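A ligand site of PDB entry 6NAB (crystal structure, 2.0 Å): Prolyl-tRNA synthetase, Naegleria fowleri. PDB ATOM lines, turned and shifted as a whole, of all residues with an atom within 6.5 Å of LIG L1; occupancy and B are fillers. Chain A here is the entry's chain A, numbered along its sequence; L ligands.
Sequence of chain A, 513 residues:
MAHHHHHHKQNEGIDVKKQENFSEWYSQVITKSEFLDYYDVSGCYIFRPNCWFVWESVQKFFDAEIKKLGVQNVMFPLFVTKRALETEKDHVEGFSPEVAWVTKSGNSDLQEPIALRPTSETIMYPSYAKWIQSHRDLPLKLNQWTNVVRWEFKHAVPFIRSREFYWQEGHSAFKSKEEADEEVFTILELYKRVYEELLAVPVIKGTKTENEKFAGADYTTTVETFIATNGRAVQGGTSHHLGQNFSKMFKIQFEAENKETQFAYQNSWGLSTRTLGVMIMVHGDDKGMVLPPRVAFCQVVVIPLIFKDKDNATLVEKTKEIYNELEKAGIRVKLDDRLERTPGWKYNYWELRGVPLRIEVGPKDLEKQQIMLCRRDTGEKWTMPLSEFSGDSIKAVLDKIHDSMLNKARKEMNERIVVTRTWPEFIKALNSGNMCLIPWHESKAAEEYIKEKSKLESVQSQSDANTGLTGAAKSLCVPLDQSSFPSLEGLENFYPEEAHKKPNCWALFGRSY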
ATOM      1  N   PHE A  95      33.741  37.146   8.233  1.00  0.00           N
ATOM      2  CA  PHE A  95      33.655  36.304   9.425  1.00  0.00           C
ATOM      3  C   PHE A  95      34.548  36.726  10.586  1.00  0.00           C
ATOM      4  O   PHE A  95      34.265  36.328  11.720  1.00  0.00           O
ATOM      5  CB  PHE A  95      33.971  34.835   9.064  1.00  0.00           C
ATOM      6  CG  PHE A  95      32.792  34.059   8.529  1.00  0.00           C
ATOM      7  CD1 PHE A  95      31.831  33.534   9.385  1.00  0.00           C
ATOM      8  CD2 PHE A  95      32.639  33.854   7.151  1.00  0.00           C
ATOM      9  CE1 PHE A  95      30.744  32.830   8.878  1.00  0.00           C
ATOM     10  CE2 PHE A  95      31.552  33.150   6.644  1.00  0.00           C
ATOM     11  CZ  PHE A  95      30.603  32.635   7.518  1.00  0.00           C
ATOM     12  N   PRO A 118      34.412  28.776  12.310  1.00  0.00           N
ATOM     13  CA  PRO A 118      33.068  29.344  12.123  1.00  0.00           C
ATOM     14  C   PRO A 118      32.327  28.664  10.973  1.00  0.00           C
ATOM     15  O   PRO A 118      31.101  28.769  10.847  1.00  0.00           O
ATOM     16  CB  PRO A 118      33.367  30.824  11.827  1.00  0.00           C
ATOM     17  CG  PRO A 118      34.652  30.739  11.043  1.00  0.00           C
ATOM     18  CD  PRO A 118      35.447  29.592  11.643  1.00  0.00           C
ATOM     19  N   THR A 119      33.084  27.956  10.132  1.00  0.00           N
ATOM     20  CA  THR A 119      32.679  27.262   8.907  1.00  0.00           C
ATOM     21  C   THR A 119      33.974  26.704   8.339  1.00  0.00           C
ATOM     22  O   THR A 119      35.059  27.157   8.701  1.00  0.00           O
ATOM     23  CB  THR A 119      31.964  28.198   7.891  1.00  0.00           C
ATOM     24  OG1 THR A 119      31.579  27.446   6.729  1.00  0.00           O
ATOM     25  CG2 THR A 119      32.873  29.342   7.454  1.00  0.00           C
ATOM     26  N   SER A 120      33.872  25.678   7.488  1.00  0.00           N
ATOM     27  CA  SER A 120      35.061  24.872   7.231  1.00  0.00           C
ATOM     28  C   SER A 120      35.649  25.004   5.827  1.00  0.00           C
ATOM     29  O   SER A 120      36.560  24.225   5.480  1.00  0.00           O
ATOM     30  CB  SER A 120      34.788  23.407   7.535  1.00  0.00           C
ATOM     31  OG  SER A 120      34.447  23.223   8.912  1.00  0.00           O
ATOM     32  N   GLU A 121      35.195  25.981   5.009  1.00  0.00           N
ATOM     33  CA  GLU A 121      35.807  26.176   3.694  1.00  0.00           C
ATOM     34  C   GLU A 121      37.339  26.242   3.770  1.00  0.00           C
ATOM     35  O   GLU A 121      38.035  25.505   3.067  1.00  0.00           O
ATOM     36  CB  GLU A 121      35.274  27.454   3.041  1.00  0.00           C
ATOM     37  CG  GLU A 121      33.884  27.308   2.391  1.00  0.00           C
ATOM     38  CD  GLU A 121      32.732  27.434   3.382  1.00  0.00           C
ATOM     39  OE1 GLU A 121      32.978  27.764   4.564  1.00  0.00           O
ATOM     40  OE2 GLU A 121      31.573  27.206   2.965  1.00  0.00           O
ATOM     41  N   ARG A 150      30.481  30.720  16.399  1.00  0.00           N
ATOM     42  CA  ARG A 150      30.421  32.064  15.861  1.00  0.00           C
ATOM     43  C   ARG A 150      30.152  33.009  17.018  1.00  0.00           C
ATOM     44  O   ARG A 150      29.106  32.918  17.666  1.00  0.00           O
ATOM     45  CB  ARG A 150      29.343  32.194  14.773  1.00  0.00           C
ATOM     46  CG  ARG A 150      29.728  31.435  13.500  1.00  0.00           C
ATOM     47  CD  ARG A 150      28.712  31.625  12.381  1.00  0.00           C
ATOM     48  NE  ARG A 150      29.005  30.677  11.306  1.00  0.00           N
ATOM     49  CZ  ARG A 150      28.379  30.616  10.128  1.00  0.00           C
ATOM     50  NH1 ARG A 150      27.402  31.473   9.827  1.00  0.00           N
ATOM     51  NH2 ARG A 150      28.746  29.685   9.265  1.00  0.00           N
ATOM     52  N   TRP A 167      25.559  21.468  13.206  1.00  0.00           N
ATOM     53  CA  TRP A 167      25.043  21.488  11.852  1.00  0.00           C
ATOM     54  C   TRP A 167      25.583  20.288  11.093  1.00  0.00           C
ATOM     55  O   TRP A 167      26.364  19.495  11.624  1.00  0.00           O
ATOM     56  CB  TRP A 167      25.388  22.823  11.157  1.00  0.00           C
ATOM     57  CG  TRP A 167      26.847  23.049  10.722  1.00  0.00           C
ATOM     58  CD1 TRP A 167      27.941  22.247  10.942  1.00  0.00           C
ATOM     59  CD2 TRP A 167      27.337  24.194   9.995  1.00  0.00           C
ATOM     60  NE1 TRP A 167      29.073  22.818  10.385  1.00  0.00           N
ATOM     61  CE2 TRP A 167      28.738  24.005   9.803  1.00  0.00           C
ATOM     62  CE3 TRP A 167      26.737  25.351   9.487  1.00  0.00           C
ATOM     63  CZ2 TRP A 167      29.529  24.948   9.129  1.00  0.00           C
ATOM     64  CZ3 TRP A 167      27.538  26.289   8.803  1.00  0.00           C
ATOM     65  CH2 TRP A 167      28.917  26.070   8.638  1.00  0.00           C
ATOM     66  N   GLN A 168      25.136  20.146   9.842  1.00  0.00           N
ATOM     67  CA  GLN A 168      25.934  19.499   8.827  1.00  0.00           C
ATOM     68  C   GLN A 168      26.380  20.576   7.837  1.00  0.00           C
ATOM     69  O   GLN A 168      25.668  21.563   7.595  1.00  0.00           O
ATOM     70  CB  GLN A 168      25.179  18.382   8.099  1.00  0.00           C
ATOM     71  CG  GLN A 168      23.838  18.809   7.408  1.00  0.00           C
ATOM     72  CD  GLN A 168      24.030  19.595   6.096  1.00  0.00           C
ATOM     73  OE1 GLN A 168      23.202  20.450   5.756  1.00  0.00           O
ATOM     74  NE2 GLN A 168      25.102  19.298   5.361  1.00  0.00           N
ATOM     75  N   GLU A 169      27.586  20.424   7.300  1.00  0.00           N
ATOM     76  CA  GLU A 169      28.060  21.259   6.205  1.00  0.00           C
ATOM     77  C   GLU A 169      28.549  20.330   5.108  1.00  0.00           C
ATOM     78  O   GLU A 169      29.413  19.469   5.368  1.00  0.00           O
ATOM     79  CB  GLU A 169      29.160  22.234   6.649  1.00  0.00           C
ATOM     80  CG  GLU A 169      30.399  21.568   7.313  1.00  0.00           C
ATOM     81  CD  GLU A 169      31.428  22.587   7.758  1.00  0.00           C
ATOM     82  OE1 GLU A 169      31.909  22.507   8.910  1.00  0.00           O
ATOM     83  OE2 GLU A 169      31.747  23.492   6.943  1.00  0.00           O
ATOM     84  N   GLY A 170      27.985  20.472   3.922  1.00  0.00           N
ATOM     85  CA  GLY A 170      28.403  19.711   2.751  1.00  0.00           C
ATOM     86  C   GLY A 170      29.255  20.593   1.855  1.00  0.00           C
ATOM     87  O   GLY A 170      28.996  21.793   1.740  1.00  0.00           O
ATOM     88  N   HIS A 171      30.289  19.995   1.261  1.00  0.00           N
ATOM     89  CA  HIS A 171      31.248  20.725   0.416  1.00  0.00           C
ATOM     90  C   HIS A 171      31.540  19.847  -0.795  1.00  0.00           C
ATOM     91  O   HIS A 171      32.141  18.779  -0.661  1.00  0.00           O
ATOM     92  CB  HIS A 171      32.545  21.037   1.165  1.00  0.00           C
ATOM     93  CG  HIS A 171      32.369  21.946   2.340  1.00  0.00           C
ATOM     94  ND1 HIS A 171      32.653  23.297   2.294  1.00  0.00           N
ATOM     95  CD2 HIS A 171      31.936  21.706   3.605  1.00  0.00           C
ATOM     96  CE1 HIS A 171      32.410  23.843   3.468  1.00  0.00           C
ATOM     97  NE2 HIS A 171      31.966  22.902   4.279  1.00  0.00           N
ATOM     98  N   TYR A 191      16.497  20.309   1.976  1.00  0.00           N
ATOM     99  CA  TYR A 191      16.212  21.163   3.131  1.00  0.00           C
ATOM    100  C   TYR A 191      14.718  21.439   3.233  1.00  0.00           C
ATOM    101  O   TYR A 191      14.136  21.394   4.325  1.00  0.00           O
ATOM    102  CB  TYR A 191      17.000  22.474   3.037  1.00  0.00           C
ATOM    103  CG  TYR A 191      18.514  22.335   3.235  1.00  0.00           C
ATOM    104  CD1 TYR A 191      19.070  21.180   3.792  1.00  0.00           C
ATOM    105  CD2 TYR A 191      19.377  23.381   2.877  1.00  0.00           C
ATOM    106  CE1 TYR A 191      20.466  21.072   4.013  1.00  0.00           C
ATOM    107  CE2 TYR A 191      20.754  23.272   3.067  1.00  0.00           C
ATOM    108  CZ  TYR A 191      21.291  22.125   3.634  1.00  0.00           C
ATOM    109  OH  TYR A 191      22.636  22.045   3.808  1.00  0.00           O
ATOM    110  N   PHE A 214      26.384  34.642   0.790  1.00  0.00           N
ATOM    111  CA  PHE A 214      27.590  34.182   1.475  1.00  0.00           C
ATOM    112  C   PHE A 214      28.831  34.826   0.864  1.00  0.00           C
ATOM    113  O   PHE A 214      28.937  34.964  -0.353  1.00  0.00           O
ATOM    114  CB  PHE A 214      27.659  32.648   1.368  1.00  0.00           C
ATOM    115  CG  PHE A 214      28.719  31.990   2.232  1.00  0.00           C
ATOM    116  CD1 PHE A 214      28.633  32.027   3.620  1.00  0.00           C
ATOM    117  CD2 PHE A 214      29.744  31.259   1.653  1.00  0.00           C
ATOM    118  CE1 PHE A 214      29.592  31.397   4.406  1.00  0.00           C
ATOM    119  CE2 PHE A 214      30.719  30.614   2.442  1.00  0.00           C
ATOM    120  CZ  PHE A 214      30.644  30.687   3.813  1.00  0.00           C
ATOM    121  N   THR A 238      20.845  27.076   4.048  1.00  0.00           N
ATOM    122  CA  THR A 238      21.347  27.732   2.845  1.00  0.00           C
ATOM    123  C   THR A 238      22.173  26.770   2.014  1.00  0.00           C
ATOM    124  O   THR A 238      22.855  25.889   2.540  1.00  0.00           O
ATOM    125  CB  THR A 238      22.207  28.963   3.175  1.00  0.00           C
ATOM    126  OG1 THR A 238      23.064  28.660   4.274  1.00  0.00           O
ATOM    127  CG2 THR A 238      21.331  30.168   3.521  1.00  0.00           C
ATOM    128  N   SER A 239      22.117  26.974   0.710  1.00  0.00           N
ATOM    129  CA  SER A 239      22.839  26.158  -0.254  1.00  0.00           C
ATOM    130  C   SER A 239      23.509  27.114  -1.227  1.00  0.00           C
ATOM    131  O   SER A 239      22.815  27.792  -1.999  1.00  0.00           O
ATOM    132  CB  SER A 239      21.894  25.177  -0.970  1.00  0.00           C
ATOM    133  OG  SER A 239      22.592  24.301  -1.840  1.00  0.00           O
ATOM    134  N   HIS A 240      24.836  27.187  -1.175  1.00  0.00           N
ATOM    135  CA  HIS A 240      25.624  28.169  -1.929  1.00  0.00           C
ATOM    136  C   HIS A 240      26.286  27.576  -3.160  1.00  0.00           C
ATOM    137  O   HIS A 240      26.875  26.488  -3.094  1.00  0.00           O
ATOM    138  CB  HIS A 240      26.742  28.783  -1.067  1.00  0.00           C
ATOM    139  CG  HIS A 240      26.331  29.165   0.310  1.00  0.00           C
ATOM    140  ND1 HIS A 240      25.453  30.204   0.566  1.00  0.00           N
ATOM    141  CD2 HIS A 240      26.735  28.704   1.516  1.00  0.00           C
ATOM    142  CE1 HIS A 240      25.314  30.327   1.875  1.00  0.00           C
ATOM    143  NE2 HIS A 240      26.084  29.444   2.474  1.00  0.00           N
ATOM    144  N   SER A 268      28.861  24.818  -1.267  1.00  0.00           N
ATOM    145  CA  SER A 268      28.782  24.394   0.119  1.00  0.00           C
ATOM    146  C   SER A 268      27.373  24.697   0.614  1.00  0.00           C
ATOM    147  O   SER A 268      26.700  25.614   0.122  1.00  0.00           O
ATOM    148  CB  SER A 268      29.864  25.069   1.019  1.00  0.00           C
ATOM    149  OG  SER A 268      29.595  26.448   1.215  1.00  0.00           O
ATOM    150  N   TRP A 269      26.909  23.897   1.570  1.00  0.00           N
ATOM    151  CA  TRP A 269      25.522  23.952   2.032  1.00  0.00           C
ATOM    152  C   TRP A 269      25.441  23.463   3.462  1.00  0.00           C
ATOM    153  O   TRP A 269      26.080  22.465   3.806  1.00  0.00           O
ATOM    154  CB  TRP A 269      24.603  23.092   1.150  1.00  0.00           C
ATOM    155  CG  TRP A 269      25.291  21.936   0.416  1.00  0.00           C
ATOM    156  CD1 TRP A 269      25.933  22.016  -0.784  1.00  0.00           C
ATOM    157  CD2 TRP A 269      25.359  20.553   0.819  1.00  0.00           C
ATOM    158  NE1 TRP A 269      26.412  20.773  -1.148  1.00  0.00           N
ATOM    159  CE2 TRP A 269      26.067  19.850  -0.187  1.00  0.00           C
ATOM    160  CE3 TRP A 269      24.885  19.829   1.933  1.00  0.00           C
ATOM    161  CZ2 TRP A 269      26.318  18.474  -0.119  1.00  0.00           C
ATOM    162  CZ3 TRP A 269      25.127  18.455   2.000  1.00  0.00           C
ATOM    163  CH2 TRP A 269      25.846  17.786   0.968  1.00  0.00           C
ATOM    164  N   GLY A 270      24.631  24.161   4.274  1.00  0.00           N
ATOM    165  CA  GLY A 270      24.549  23.906   5.698  1.00  0.00           C
ATOM    166  C   GLY A 270      23.155  24.044   6.307  1.00  0.00           C
ATOM    167  O   GLY A 270      22.386  24.952   5.948  1.00  0.00           O
ATOM    168  N   LEU A 271      22.836  23.124   7.207  1.00  0.00           N
ATOM    169  CA  LEU A 271      21.579  23.088   7.963  1.00  0.00           C
ATOM    170  C   LEU A 271      21.954  22.867   9.427  1.00  0.00           C
ATOM    171  O   LEU A 271      22.770  21.997   9.729  1.00  0.00           O
ATOM    172  CB  LEU A 271      20.684  21.945   7.483  1.00  0.00           C
ATOM    173  CG  LEU A 271      19.290  21.840   8.099  1.00  0.00           C
ATOM    174  CD1 LEU A 271      18.380  22.875   7.448  1.00  0.00           C
ATOM    175  CD2 LEU A 271      18.737  20.443   7.906  1.00  0.00           C
HETATM  176  N1  LIG L   1      29.603  27.048   4.858  1.00  0.00           N
HETATM  177  C1  LIG L   1      28.394  27.715   4.357  1.00  0.00           C
HETATM  178  C2  LIG L   1      27.851  28.664   5.419  1.00  0.00           C
HETATM  179  O1  LIG L   1      28.458  28.778   6.504  1.00  0.00           O
HETATM  180  C3  LIG L   1      27.415  26.555   4.093  1.00  0.00           C
HETATM  181  C4  LIG L   1      27.887  25.460   5.046  1.00  0.00           C
HETATM  182  C5  LIG L   1      29.393  25.598   5.067  1.00  0.00           C
HETATM  183  O2  LIG L   1      26.828  29.320   5.218  1.00  0.00           O
HETATM  184  P1  LG2 L   2      24.727  31.304   6.956  1.00  0.00           P
HETATM  185  O1  LG2 L   2      24.237  32.555   7.674  1.00  0.00           O
HETATM  186  O2  LG2 L   2      26.327  31.101   6.851  1.00  0.00           O
HETATM  187  O3  LG2 L   2      24.110  31.081   5.556  1.00  0.00           O
HETATM  188  O4  LG2 L   2      24.166  30.084   7.789  1.00  0.00           O
HETATM  189  C1  LG2 L   2      24.549  28.743   7.474  1.00  0.00           C
HETATM  190  C2  LG2 L   2      23.754  27.749   8.270  1.00  0.00           C
HETATM  191  O5  LG2 L   2      24.044  27.929   9.686  1.00  0.00           O
HETATM  192  C3  LG2 L   2      22.240  27.869   8.138  1.00  0.00           C
HETATM  193  O6  LG2 L   2      21.663  26.573   8.272  1.00  0.00           O
HETATM  194  C4  LG2 L   2      21.851  28.731   9.330  1.00  0.00           C
HETATM  195  O7  LG2 L   2      20.520  28.549   9.758  1.00  0.00           O
HETATM  196  C5  LG2 L   2      22.863  28.275  10.389  1.00  0.00           C
HETATM  197  N1  LG2 L   2      23.240  29.275  11.390  1.00  0.00           N
HETATM  198  C6  LG2 L   2      23.993  30.405  11.178  1.00  0.00           C
HETATM  199  N2  LG2 L   2      24.301  31.062  12.276  1.00  0.00           N
HETATM  200  C7  LG2 L   2      23.702  30.313  13.282  1.00  0.00           C
HETATM  201  C8  LG2 L   2      23.679  30.460  14.679  1.00  0.00           C
HETATM  202  N3  LG2 L   2      24.322  31.430  15.343  1.00  0.00           N
HETATM  203  N4  LG2 L   2      22.994  29.535  15.402  1.00  0.00           N
HETATM  204  C9  LG2 L   2      22.403  28.529  14.746  1.00  0.00           C
HETATM  205  N5  LG2 L   2      22.361  28.290  13.427  1.00  0.00           N
HETATM  206  C10 LG2 L   2      23.033  29.218  12.754  1.00  0.00           C
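OE2 of Glu 121 lies within salt-bridge range of N1 of LIG L1 (2.7 Å).
The side-chain hydroxyl of Thr 119 lies within hydrogen-bond range of a nitrogen (N1) of LIG L1, 2.8 Å away.
A ring nitrogen (NE2) of His 240 sits at hydrogen-bond distance from an oxygen (O2) of LIG L1 (2.8 Å).
The guanidinium group of Arg 150 lies within salt-bridge range of an oxygen (O1) of LIG L1 (2.9 Å).
The guanidinium group of Arg 150 is in salt-bridge range of an oxygen (O2) of LG2 L2, at 3.2 Å.
An oxygen (O6) of LG2 L2 is in hydrogen-bond range of the backbone carbonyl oxygen (O) of Gly 270 (2.9 Å).
OG1 of Thr 238 sits at hydrogen-bond distance from O3 of LG2 L2 (2.9 Å).
OE1 of Glu 121 sits at hydrogen-bond distance from OG1 of Thr 119 (2.6 Å).
The backbone NH (N) of His 240 sits at hydrogen-bond distance from the backbone carbonyl oxygen (O) of Ser 268 (2.8 Å).
O of Pro 118 sits at hydrogen-bond distance from NE of Arg 150 (2.9 Å).
The indole nitrogen (NE1) of Trp 167 is in hydrogen-bond range of the side-chain carboxylate (OE1) of Glu 169 (3.2 Å).
The backbone carbonyl oxygen (O) of Trp 269 lies within hydrogen-bond range of the backbone NH (N) of Gly 170, at 2.8 Å.
N of Gly 270 sits at hydrogen-bond distance from O of Thr 238.
The backbone NH (N) of Gly 270 lies within hydrogen-bond range of the side-chain hydroxyl (OH) of Tyr 191 (2.9 Å).
OE1 of Glu 169 lies within hydrogen-bond range of OG of Ser 120, at 2.6 Å.
O2 of LIG L1 sits close to O2 of LG2 L2.
CH2 of Trp 167 touches O1 of LIG L1, 3.5 Å away.
Glu 169 touches LIG L1.
NE2 of His 171 touches C5 of LIG L1, at 3.8 Å.
Phe 214 touches LIG L1 (CE1 to C2, 3.4 Å).
Thr 238 touches LIG L1.
Ser 268 touches LIG L1.
C of Trp 269 touches C4 of LIG L1, at 3.5 Å.
N of Gly 270 touches C4 of LIG L1, at 3.6 Å.
Hydrophobic or aromatic side chains that line LIG L1: Trp 167, His 171, Phe 214 and His 240.
The nearest printed residue that does not touch LIG L1 is Phe 95 (4.5 Å).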
